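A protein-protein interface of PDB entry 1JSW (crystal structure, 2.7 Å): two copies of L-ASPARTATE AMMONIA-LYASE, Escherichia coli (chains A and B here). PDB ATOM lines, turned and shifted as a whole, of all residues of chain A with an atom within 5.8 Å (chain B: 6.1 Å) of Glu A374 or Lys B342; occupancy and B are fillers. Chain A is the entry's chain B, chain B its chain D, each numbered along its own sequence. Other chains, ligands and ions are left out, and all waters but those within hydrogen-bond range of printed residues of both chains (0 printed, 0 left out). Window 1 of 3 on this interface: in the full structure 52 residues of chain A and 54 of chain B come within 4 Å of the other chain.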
ATOM      1  N   TYR A  98     -16.072  -3.719  -6.612  1.00  0.00           N
ATOM      2  CA  TYR A  98     -15.521  -2.475  -7.151  1.00  0.00           C
ATOM      3  C   TYR A  98     -14.016  -2.597  -6.950  1.00  0.00           C
ATOM      4  O   TYR A  98     -13.551  -2.881  -5.846  1.00  0.00           O
ATOM      5  CB  TYR A  98     -16.037  -1.254  -6.378  1.00  0.00           C
ATOM      6  CG  TYR A  98     -17.509  -0.988  -6.554  1.00  0.00           C
ATOM      7  CD1 TYR A  98     -18.453  -1.649  -5.773  1.00  0.00           C
ATOM      8  CD2 TYR A  98     -17.963  -0.090  -7.515  1.00  0.00           C
ATOM      9  CE1 TYR A  98     -19.807  -1.427  -5.944  1.00  0.00           C
ATOM     10  CE2 TYR A  98     -19.318   0.139  -7.697  1.00  0.00           C
ATOM     11  CZ  TYR A  98     -20.232  -0.534  -6.908  1.00  0.00           C
ATOM     12  OH  TYR A  98     -21.577  -0.326  -7.091  1.00  0.00           O
ATOM     13  N   LYS A 342     -34.185  -1.846 -12.030  1.00  0.00           N
ATOM     14  CA  LYS A 342     -32.792  -1.916 -11.622  1.00  0.00           C
ATOM     15  C   LYS A 342     -32.022  -2.489 -12.793  1.00  0.00           C
ATOM     16  O   LYS A 342     -31.052  -1.901 -13.247  1.00  0.00           O
ATOM     17  CB  LYS A 342     -32.661  -2.809 -10.374  1.00  0.00           C
ATOM     18  CG  LYS A 342     -31.266  -2.895  -9.754  1.00  0.00           C
ATOM     19  CD  LYS A 342     -30.776  -1.565  -9.211  1.00  0.00           C
ATOM     20  CE  LYS A 342     -29.383  -1.707  -8.635  1.00  0.00           C
ATOM     21  NZ  LYS A 342     -28.830  -0.405  -8.201  1.00  0.00           N
ATOM     22  N   ASN A 346     -29.022  -0.762 -14.905  1.00  0.00           N
ATOM     23  CA  ASN A 346     -27.660  -1.290 -14.951  1.00  0.00           C
ATOM     24  C   ASN A 346     -27.110  -1.155 -16.364  1.00  0.00           C
ATOM     25  O   ASN A 346     -25.895  -1.124 -16.571  1.00  0.00           O
ATOM     26  CB  ASN A 346     -27.624  -2.759 -14.536  1.00  0.00           C
ATOM     27  CG  ASN A 346     -27.573  -2.942 -13.038  1.00  0.00           C
ATOM     28  OD1 ASN A 346     -27.609  -4.069 -12.544  1.00  0.00           O
ATOM     29  ND2 ASN A 346     -27.467  -1.837 -12.302  1.00  0.00           N
ATOM     30  N   THR A 349     -25.180   1.874 -16.918  1.00  0.00           N
ATOM     31  CA  THR A 349     -23.868   1.810 -16.282  1.00  0.00           C
ATOM     32  C   THR A 349     -22.865   1.264 -17.288  1.00  0.00           C
ATOM     33  O   THR A 349     -22.002   1.997 -17.770  1.00  0.00           O
ATOM     34  CB  THR A 349     -23.876   0.862 -15.068  1.00  0.00           C
ATOM     35  OG1 THR A 349     -24.866   1.283 -14.118  1.00  0.00           O
ATOM     36  CG2 THR A 349     -22.511   0.821 -14.428  1.00  0.00           C
ATOM     37  N   VAL A 367     -16.679  -3.118 -13.716  1.00  0.00           N
ATOM     38  CA  VAL A 367     -17.913  -2.424 -13.385  1.00  0.00           C
ATOM     39  C   VAL A 367     -18.961  -3.042 -14.274  1.00  0.00           C
ATOM     40  O   VAL A 367     -20.120  -3.137 -13.900  1.00  0.00           O
ATOM     41  CB  VAL A 367     -17.829  -0.904 -13.618  1.00  0.00           C
ATOM     42  CG1 VAL A 367     -17.997  -0.574 -15.075  1.00  0.00           C
ATOM     43  CG2 VAL A 367     -18.870  -0.198 -12.792  1.00  0.00           C
ATOM     44  N   GLY A 369     -18.754  -6.030 -15.056  1.00  0.00           N
ATOM     45  CA  GLY A 369     -18.892  -7.345 -14.451  1.00  0.00           C
ATOM     46  C   GLY A 369     -19.988  -7.491 -13.409  1.00  0.00           C
ATOM     47  O   GLY A 369     -20.912  -8.292 -13.581  1.00  0.00           O
ATOM     48  N   GLN A 370     -19.893  -6.718 -12.327  1.00  0.00           N
ATOM     49  CA  GLN A 370     -20.887  -6.786 -11.256  1.00  0.00           C
ATOM     50  C   GLN A 370     -22.227  -6.245 -11.718  1.00  0.00           C
ATOM     51  O   GLN A 370     -23.267  -6.641 -11.207  1.00  0.00           O
ATOM     52  CB  GLN A 370     -20.397  -6.034 -10.015  1.00  0.00           C
ATOM     53  CG  GLN A 370     -20.628  -4.526 -10.018  1.00  0.00           C
ATOM     54  CD  GLN A 370     -21.859  -4.124  -9.218  1.00  0.00           C
ATOM     55  OE1 GLN A 370     -22.845  -3.628  -9.774  1.00  0.00           O
ATOM     56  NE2 GLN A 370     -21.810  -4.341  -7.905  1.00  0.00           N
ATOM     57  N   ALA A 371     -22.186  -5.315 -12.666  1.00  0.00           N
ATOM     58  CA  ALA A 371     -23.397  -4.745 -13.218  1.00  0.00           C
ATOM     59  C   ALA A 371     -24.077  -5.854 -13.988  1.00  0.00           C
ATOM     60  O   ALA A 371     -25.259  -6.127 -13.795  1.00  0.00           O
ATOM     61  CB  ALA A 371     -23.063  -3.616 -14.153  1.00  0.00           C
ATOM     62  N   MET A 372     -23.306  -6.498 -14.857  1.00  0.00           N
ATOM     63  CA  MET A 372     -23.804  -7.595 -15.675  1.00  0.00           C
ATOM     64  C   MET A 372     -24.346  -8.656 -14.738  1.00  0.00           C
ATOM     65  O   MET A 372     -25.546  -8.916 -14.721  1.00  0.00           O
ATOM     66  CB  MET A 372     -22.666  -8.175 -16.523  1.00  0.00           C
ATOM     67  CG  MET A 372     -23.063  -9.269 -17.494  1.00  0.00           C
ATOM     68  SD  MET A 372     -23.846  -8.656 -18.978  1.00  0.00           S
ATOM     69  CE  MET A 372     -22.612  -7.497 -19.517  1.00  0.00           C
ATOM     70  N   PHE A 373     -23.458  -9.207 -13.911  1.00  0.00           N
ATOM     71  CA  PHE A 373     -23.799 -10.246 -12.948  1.00  0.00           C
ATOM     72  C   PHE A 373     -25.033  -9.943 -12.104  1.00  0.00           C
ATOM     73  O   PHE A 373     -25.892 -10.811 -11.918  1.00  0.00           O
ATOM     74  CB  PHE A 373     -22.599 -10.540 -12.053  1.00  0.00           C
ATOM     75  CG  PHE A 373     -21.572 -11.411 -12.704  1.00  0.00           C
ATOM     76  CD1 PHE A 373     -21.940 -12.608 -13.300  1.00  0.00           C
ATOM     77  CD2 PHE A 373     -20.242 -11.029 -12.745  1.00  0.00           C
ATOM     78  CE1 PHE A 373     -21.004 -13.409 -13.927  1.00  0.00           C
ATOM     79  CE2 PHE A 373     -19.300 -11.828 -13.373  1.00  0.00           C
ATOM     80  CZ  PHE A 373     -19.683 -13.017 -13.963  1.00  0.00           C
ATOM     81  N   GLU A 374     -25.117  -8.710 -11.610  1.00  0.00           N
ATOM     82  CA  GLU A 374     -26.246  -8.258 -10.804  1.00  0.00           C
ATOM     83  C   GLU A 374     -27.555  -8.623 -11.522  1.00  0.00           C
ATOM     84  O   GLU A 374     -28.335  -9.430 -11.014  1.00  0.00           O
ATOM     85  CB  GLU A 374     -26.145  -6.739 -10.600  1.00  0.00           C
ATOM     86  CG  GLU A 374     -26.926  -6.144  -9.429  1.00  0.00           C
ATOM     87  CD  GLU A 374     -26.542  -4.685  -9.161  1.00  0.00           C
ATOM     88  OE1 GLU A 374     -26.809  -3.820 -10.023  1.00  0.00           O
ATOM     89  OE2 GLU A 374     -25.961  -4.392  -8.091  1.00  0.00           O
ATOM     90  N   SER A 375     -27.738  -8.124 -12.747  1.00  0.00           N
ATOM     91  CA  SER A 375     -28.963  -8.387 -13.508  1.00  0.00           C
ATOM     92  C   SER A 375     -29.318  -9.833 -13.733  1.00  0.00           C
ATOM     93  O   SER A 375     -30.471 -10.220 -13.597  1.00  0.00           O
ATOM     94  CB  SER A 375     -28.959  -7.645 -14.828  1.00  0.00           C
ATOM     95  OG  SER A 375     -29.235  -6.283 -14.582  1.00  0.00           O
ATOM     96  N   VAL A 376     -28.337 -10.630 -14.106  1.00  0.00           N
ATOM     97  CA  VAL A 376     -28.596 -12.033 -14.317  1.00  0.00           C
ATOM     98  C   VAL A 376     -29.153 -12.588 -13.010  1.00  0.00           C
ATOM     99  O   VAL A 376     -30.207 -13.216 -12.996  1.00  0.00           O
ATOM    100  CB  VAL A 376     -27.302 -12.765 -14.698  1.00  0.00           C
ATOM    101  CG1 VAL A 376     -27.508 -14.281 -14.640  1.00  0.00           C
ATOM    102  CG2 VAL A 376     -26.851 -12.320 -16.088  1.00  0.00           C
ATOM    103  N   HIS A 377     -28.494 -12.250 -11.907  1.00  0.00           N
ATOM    104  CA  HIS A 377     -28.886 -12.709 -10.583  1.00  0.00           C
ATOM    105  C   HIS A 377     -30.327 -12.365 -10.191  1.00  0.00           C
ATOM    106  O   HIS A 377     -31.145 -13.257  -9.968  1.00  0.00           O
ATOM    107  CB  HIS A 377     -27.898 -12.154  -9.546  1.00  0.00           C
ATOM    108  CG  HIS A 377     -28.155 -12.610  -8.138  1.00  0.00           C
ATOM    109  ND1 HIS A 377     -28.386 -11.728  -7.103  1.00  0.00           N
ATOM    110  CD2 HIS A 377     -28.172 -13.846  -7.587  1.00  0.00           C
ATOM    111  CE1 HIS A 377     -28.531 -12.403  -5.976  1.00  0.00           C
ATOM    112  NE2 HIS A 377     -28.405 -13.691  -6.242  1.00  0.00           N
ATOM    113  N   ILE A 378     -30.633 -11.073 -10.111  1.00  0.00           N
ATOM    114  CA  ILE A 378     -31.962 -10.602  -9.716  1.00  0.00           C
ATOM    115  C   ILE A 378     -33.091 -11.044 -10.642  1.00  0.00           C
ATOM    116  O   ILE A 378     -34.186 -11.370 -10.195  1.00  0.00           O
ATOM    117  CB  ILE A 378     -31.967  -9.075  -9.551  1.00  0.00           C
ATOM    118  CG1 ILE A 378     -31.550  -8.398 -10.856  1.00  0.00           C
ATOM    119  CG2 ILE A 378     -31.001  -8.671  -8.441  1.00  0.00           C
ATOM    120  CD1 ILE A 378     -31.299  -6.909 -10.718  1.00  0.00           C
ATOM    121  N   LEU A 379     -32.814 -11.050 -11.939  1.00  0.00           N
ATOM    122  CA  LEU A 379     -33.786 -11.490 -12.924  1.00  0.00           C
ATOM    123  C   LEU A 379     -34.199 -12.912 -12.583  1.00  0.00           C
ATOM    124  O   LEU A 379     -35.374 -13.192 -12.386  1.00  0.00           O
ATOM    125  CB  LEU A 379     -33.180 -11.438 -14.329  1.00  0.00           C
ATOM    126  CG  LEU A 379     -33.001 -10.029 -14.900  1.00  0.00           C
ATOM    127  CD1 LEU A 379     -32.262 -10.064 -16.219  1.00  0.00           C
ATOM    128  CD2 LEU A 379     -34.358  -9.396 -15.063  1.00  0.00           C
ATOM    129  N   TYR B  98     -35.630  -5.211  -2.076  1.00  0.00           N
ATOM    130  CA  TYR B  98     -36.525  -5.266  -3.222  1.00  0.00           C
ATOM    131  C   TYR B  98     -37.783  -5.820  -2.615  1.00  0.00           C
ATOM    132  O   TYR B  98     -37.794  -6.956  -2.149  1.00  0.00           O
ATOM    133  CB  TYR B  98     -36.032  -6.258  -4.279  1.00  0.00           C
ATOM    134  CG  TYR B  98     -34.767  -5.868  -4.996  1.00  0.00           C
ATOM    135  CD1 TYR B  98     -34.794  -5.008  -6.087  1.00  0.00           C
ATOM    136  CD2 TYR B  98     -33.541  -6.388  -4.599  1.00  0.00           C
ATOM    137  CE1 TYR B  98     -33.634  -4.690  -6.769  1.00  0.00           C
ATOM    138  CE2 TYR B  98     -32.377  -6.076  -5.270  1.00  0.00           C
ATOM    139  CZ  TYR B  98     -32.425  -5.230  -6.348  1.00  0.00           C
ATOM    140  OH  TYR B  98     -31.251  -4.938  -7.001  1.00  0.00           O
ATOM    141  N   HIS B 281     -31.643  12.097  -5.907  1.00  0.00           N
ATOM    142  CA  HIS B 281     -30.767  11.141  -6.551  1.00  0.00           C
ATOM    143  C   HIS B 281     -30.120  11.775  -7.767  1.00  0.00           C
ATOM    144  O   HIS B 281     -28.997  11.432  -8.128  1.00  0.00           O
ATOM    145  CB  HIS B 281     -31.481   9.858  -6.934  1.00  0.00           C
ATOM    146  CG  HIS B 281     -30.537   8.759  -7.304  1.00  0.00           C
ATOM    147  ND1 HIS B 281     -29.421   8.971  -8.079  1.00  0.00           N
ATOM    148  CD2 HIS B 281     -30.515   7.450  -6.964  1.00  0.00           C
ATOM    149  CE1 HIS B 281     -28.746   7.841  -8.201  1.00  0.00           C
ATOM    150  NE2 HIS B 281     -29.388   6.904  -7.534  1.00  0.00           N
ATOM    151  N   ASN B 337     -14.414   5.863 -10.827  1.00  0.00           N
ATOM    152  CA  ASN B 337     -15.177   5.978 -12.060  1.00  0.00           C
ATOM    153  C   ASN B 337     -16.252   4.906 -12.031  1.00  0.00           C
ATOM    154  O   ASN B 337     -17.425   5.200 -12.244  1.00  0.00           O
ATOM    155  CB  ASN B 337     -14.291   5.783 -13.292  1.00  0.00           C
ATOM    156  CG  ASN B 337     -13.436   6.998 -13.606  1.00  0.00           C
ATOM    157  OD1 ASN B 337     -12.256   6.874 -13.929  1.00  0.00           O
ATOM    158  ND2 ASN B 337     -14.035   8.174 -13.546  1.00  0.00           N
ATOM    159  N   GLN B 338     -15.860   3.681 -11.692  1.00  0.00           N
ATOM    160  CA  GLN B 338     -16.795   2.556 -11.648  1.00  0.00           C
ATOM    161  C   GLN B 338     -18.004   2.786 -10.768  1.00  0.00           C
ATOM    162  O   GLN B 338     -19.123   2.442 -11.150  1.00  0.00           O
ATOM    163  CB  GLN B 338     -16.077   1.288 -11.227  1.00  0.00           C
ATOM    164  CG  GLN B 338     -14.928   0.987 -12.136  1.00  0.00           C
ATOM    165  CD  GLN B 338     -14.192  -0.252 -11.752  1.00  0.00           C
ATOM    166  OE1 GLN B 338     -13.040  -0.442 -12.140  1.00  0.00           O
ATOM    167  NE2 GLN B 338     -14.849  -1.119 -10.992  1.00  0.00           N
ATOM    168  N   VAL B 339     -17.790   3.373  -9.597  1.00  0.00           N
ATOM    169  CA  VAL B 339     -18.913   3.632  -8.717  1.00  0.00           C
ATOM    170  C   VAL B 339     -19.776   4.728  -9.340  1.00  0.00           C
ATOM    171  O   VAL B 339     -20.989   4.564  -9.480  1.00  0.00           O
ATOM    172  CB  VAL B 339     -18.470   3.985  -7.256  1.00  0.00           C
ATOM    173  CG1 VAL B 339     -17.292   3.122  -6.852  1.00  0.00           C
ATOM    174  CG2 VAL B 339     -18.163   5.466  -7.078  1.00  0.00           C
ATOM    175  N   CYS B 340     -19.132   5.797  -9.803  1.00  0.00           N
ATOM    176  CA  CYS B 340     -19.843   6.908 -10.422  1.00  0.00           C
ATOM    177  C   CYS B 340     -20.815   6.331 -11.436  1.00  0.00           C
ATOM    178  O   CYS B 340     -22.013   6.597 -11.372  1.00  0.00           O
ATOM    179  CB  CYS B 340     -18.867   7.849 -11.128  1.00  0.00           C
ATOM    180  SG  CYS B 340     -17.597   8.577 -10.066  1.00  0.00           S
ATOM    181  N   PHE B 341     -20.303   5.443 -12.288  1.00  0.00           N
ATOM    182  CA  PHE B 341     -21.099   4.789 -13.321  1.00  0.00           C
ATOM    183  C   PHE B 341     -22.354   4.124 -12.752  1.00  0.00           C
ATOM    184  O   PHE B 341     -23.412   4.162 -13.378  1.00  0.00           O
ATOM    185  CB  PHE B 341     -20.254   3.751 -14.070  1.00  0.00           C
ATOM    186  CG  PHE B 341     -19.044   4.320 -14.757  1.00  0.00           C
ATOM    187  CD1 PHE B 341     -18.991   5.656 -15.124  1.00  0.00           C
ATOM    188  CD2 PHE B 341     -17.946   3.520 -15.019  1.00  0.00           C
ATOM    189  CE1 PHE B 341     -17.857   6.190 -15.741  1.00  0.00           C
ATOM    190  CE2 PHE B 341     -16.814   4.046 -15.632  1.00  0.00           C
ATOM    191  CZ  PHE B 341     -16.773   5.387 -15.993  1.00  0.00           C
ATOM    192  N   LYS B 342     -22.251   3.538 -11.561  1.00  0.00           N
ATOM    193  CA  LYS B 342     -23.405   2.879 -10.961  1.00  0.00           C
ATOM    194  C   LYS B 342     -24.436   3.908 -10.521  1.00  0.00           C
ATOM    195  O   LYS B 342     -25.635   3.709 -10.703  1.00  0.00           O
ATOM    196  CB  LYS B 342     -22.996   2.016  -9.768  1.00  0.00           C
ATOM    197  CG  LYS B 342     -24.065   1.018  -9.308  1.00  0.00           C
ATOM    198  CD  LYS B 342     -23.967  -0.299 -10.061  1.00  0.00           C
ATOM    199  CE  LYS B 342     -24.726  -1.413  -9.371  1.00  0.00           C
ATOM    200  NZ  LYS B 342     -26.183  -1.179  -9.331  1.00  0.00           N
ATOM    201  N   VAL B 343     -23.969   5.011  -9.949  1.00  0.00           N
ATOM    202  CA  VAL B 343     -24.869   6.061  -9.481  1.00  0.00           C
ATOM    203  C   VAL B 343     -25.752   6.510 -10.623  1.00  0.00           C
ATOM    204  O   VAL B 343     -26.983   6.576 -10.503  1.00  0.00           O
ATOM    205  CB  VAL B 343     -24.076   7.266  -8.964  1.00  0.00           C
ATOM    206  CG1 VAL B 343     -24.984   8.474  -8.790  1.00  0.00           C
ATOM    207  CG2 VAL B 343     -23.416   6.909  -7.657  1.00  0.00           C
ATOM    208  N   ILE B 344     -25.080   6.803 -11.731  1.00  0.00           N
ATOM    209  CA  ILE B 344     -25.689   7.251 -12.967  1.00  0.00           C
ATOM    210  C   ILE B 344     -26.671   6.172 -13.426  1.00  0.00           C
ATOM    211  O   ILE B 344     -27.768   6.470 -13.895  1.00  0.00           O
ATOM    212  CB  ILE B 344     -24.570   7.509 -14.003  1.00  0.00           C
ATOM    213  CG1 ILE B 344     -23.700   8.677 -13.523  1.00  0.00           C
ATOM    214  CG2 ILE B 344     -25.147   7.756 -15.388  1.00  0.00           C
ATOM    215  CD1 ILE B 344     -22.436   8.905 -14.322  1.00  0.00           C
ATOM    216  N   GLY B 345     -26.288   4.915 -13.236  1.00  0.00           N
ATOM    217  CA  GLY B 345     -27.157   3.822 -13.607  1.00  0.00           C
ATOM    218  C   GLY B 345     -28.301   3.743 -12.613  1.00  0.00           C
ATOM    219  O   GLY B 345     -29.417   3.362 -12.969  1.00  0.00           O
ATOM    220  N   ASN B 346     -28.030   4.105 -11.360  1.00  0.00           N
ATOM    221  CA  ASN B 346     -29.055   4.088 -10.316  1.00  0.00           C
ATOM    222  C   ASN B 346     -30.036   5.245 -10.473  1.00  0.00           C
ATOM    223  O   ASN B 346     -31.028   5.332  -9.738  1.00  0.00           O
ATOM    224  CB  ASN B 346     -28.418   4.144  -8.939  1.00  0.00           C
ATOM    225  CG  ASN B 346     -27.709   2.878  -8.586  1.00  0.00           C
ATOM    226  OD1 ASN B 346     -27.911   1.836  -9.208  1.00  0.00           O
ATOM    227  ND2 ASN B 346     -26.866   2.949  -7.577  1.00  0.00           N
ATOM    228  N   ASP B 347     -29.748   6.119 -11.440  1.00  0.00           N
ATOM    229  CA  ASP B 347     -30.570   7.286 -11.749  1.00  0.00           C
ATOM    230  C   ASP B 347     -31.737   6.959 -12.705  1.00  0.00           C
ATOM    231  O   ASP B 347     -32.826   7.524 -12.587  1.00  0.00           O
ATOM    232  CB  ASP B 347     -29.678   8.378 -12.331  1.00  0.00           C
ATOM    233  CG  ASP B 347     -30.433   9.629 -12.647  1.00  0.00           C
ATOM    234  OD1 ASP B 347     -30.966   9.730 -13.773  1.00  0.00           O
ATOM    235  OD2 ASP B 347     -30.484  10.523 -11.785  1.00  0.00           O
ATOM    236  N   GLU B 374     -27.740   2.923  -2.197  1.00  0.00           N
ATOM    237  CA  GLU B 374     -26.582   2.364  -2.871  1.00  0.00           C
ATOM    238  C   GLU B 374     -25.657   3.511  -3.297  1.00  0.00           C
ATOM    239  O   GLU B 374     -24.451   3.467  -3.048  1.00  0.00           O
ATOM    240  CB  GLU B 374     -27.047   1.576  -4.094  1.00  0.00           C
ATOM    241  CG  GLU B 374     -25.999   0.695  -4.764  1.00  0.00           C
ATOM    242  CD  GLU B 374     -26.580  -0.077  -5.938  1.00  0.00           C
ATOM    243  OE1 GLU B 374     -27.120  -1.185  -5.732  1.00  0.00           O
ATOM    244  OE2 GLU B 374     -26.523   0.433  -7.072  1.00  0.00           O
ATOM    245  N   SER B 375     -26.249   4.564  -3.864  1.00  0.00           N
ATOM    246  CA  SER B 375     -25.512   5.741  -4.333  1.00  0.00           C
ATOM    247  C   SER B 375     -24.847   6.566  -3.230  1.00  0.00           C
ATOM    248  O   SER B 375     -23.685   6.962  -3.362  1.00  0.00           O
ATOM    249  CB  SER B 375     -26.426   6.650  -5.157  1.00  0.00           C
ATOM    250  OG  SER B 375     -26.910   5.988  -6.307  1.00  0.00           O
ATOM    251  N   ILE B 378     -21.788   4.226  -1.786  1.00  0.00           N
ATOM    252  CA  ILE B 378     -20.555   4.186  -2.575  1.00  0.00           C
ATOM    253  C   ILE B 378     -19.950   5.534  -2.885  1.00  0.00           C
ATOM    254  O   ILE B 378     -18.751   5.620  -3.096  1.00  0.00           O
ATOM    255  CB  ILE B 378     -20.690   3.366  -3.891  1.00  0.00           C
ATOM    256  CG1 ILE B 378     -21.664   4.027  -4.870  1.00  0.00           C
ATOM    257  CG2 ILE B 378     -21.136   1.938  -3.577  1.00  0.00           C
ATOM    258  CD1 ILE B 378     -21.966   3.175  -6.099  1.00  0.00           C
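Of the 16 printed residues of chain A, 7 touch a printed residue of chain B. Hydrophobic or aromatic side chains of chain A that line the printed part of chain B: Tyr A98 and Val A367. Of the 16 printed residues of chain B, 9 touch a printed residue of chain A. Printed residues of chain B that touch a printed residue of chain A: Tyr B98, Gln B338, Val B339, Phe B341, Lys B342, Gly B345, Asn B346, Glu B374 and Ile B378. Hydrophobic or aromatic side chains of chain B that line the printed part of chain A: Tyr B98, Val B339, Phe B341 and Ile B378. Among the printed residues, Asp or Glu carboxylates within 4 Å of a Lys or Arg side-chain nitrogen of the other chain: Lys A342 with Glu B374 (2.7 Å) and Glu A374 with Lys B342 (2.8 Å).
Met A372 touches none of the printed residues of chain B. Glu A374 touches just one residue of chain B: Lys B342 (2.8 Å). Of the printed residues of chain A, Tyr B98 touches Lys A342. Lys B342 touches six residues of chain A. Of the printed residues of chain A, Glu B374 touches Lys A342 (2.7 Å).
The side-chain amino group (NZ) of Lys A342 is in hydrogen-bond range of the side-chain amide oxygen (OD1) of Asn B346, at 2.6 Å. The side-chain carboxylate of Glu B374 is in salt-bridge range of the side-chain amino group of Lys A342, 2.7 Å away. NZ of Lys B342 sits close to ND2 of Asn A346 (3.3 Å). The side-chain hydroxyl (OG1) of Thr A349 lies within hydrogen-bond range of the backbone carbonyl oxygen (O) of Phe B341 (3.3 Å). NZ of Lys B342 is in salt-bridge range of OE1 of Glu A374 (2.8 Å). NZ of Lys A342 lies close to NZ of Lys B342 (3.0 Å).
The backbone carbonyl oxygen (O) of Ala A371 sits close to the side-chain amide oxygen (OD1) of Asn A346, at 3.4 Å. OE1 of Glu A374 lies close to OD1 of Asn A346. OD1 of Asn B346 sits close to O of Lys B342, 3.3 Å away. OE2 of Glu B374 is in salt-bridge range of NZ of Lys B342 (2.8 Å). The side-chain amide nitrogen of Asn B346 sits at hydrogen-bond distance from the side-chain carboxylate of Glu B374 (2.6 Å). The side-chain amide nitrogen of Asn B346 lies within hydrogen-bond range of the side-chain hydroxyl of Ser B375 (3.3 Å).
CD2 of Tyr A98 touches CG1 of Val B339, at 3.3 Å. Tyr A98 touches Lys B342 (OH to CG, 3.6 Å). Tyr A98 touches Ile B378 (OH to CD1, 3.7 Å). Lys A342 touches Tyr B98. Thr A349 touches Lys B342. OG1 of Thr A349 touches CA of Gly B345 (3.5 Å). Val A367 touches Gln B338. Gln A370 touches Lys B342 (OE1 to CE, 2.9 Å).
Tyr A98 touches Lys B342, and with the chains exchanged Lys A342 touches Tyr B98. Tyr A98 touches Ile B378, but with the chains exchanged Ile A378 does not touch Tyr B98 (4.01 Å). Lys A342 touches its own counterpart, Lys B342. Lys A342 touches Glu B374, and with the chains exchanged Glu A374 touches Lys B342. 6 positions are printed for both chains. Of the 14 pairs that touch across the chains among the printed residues, 7 have their exchanged pair printed and touching as well.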
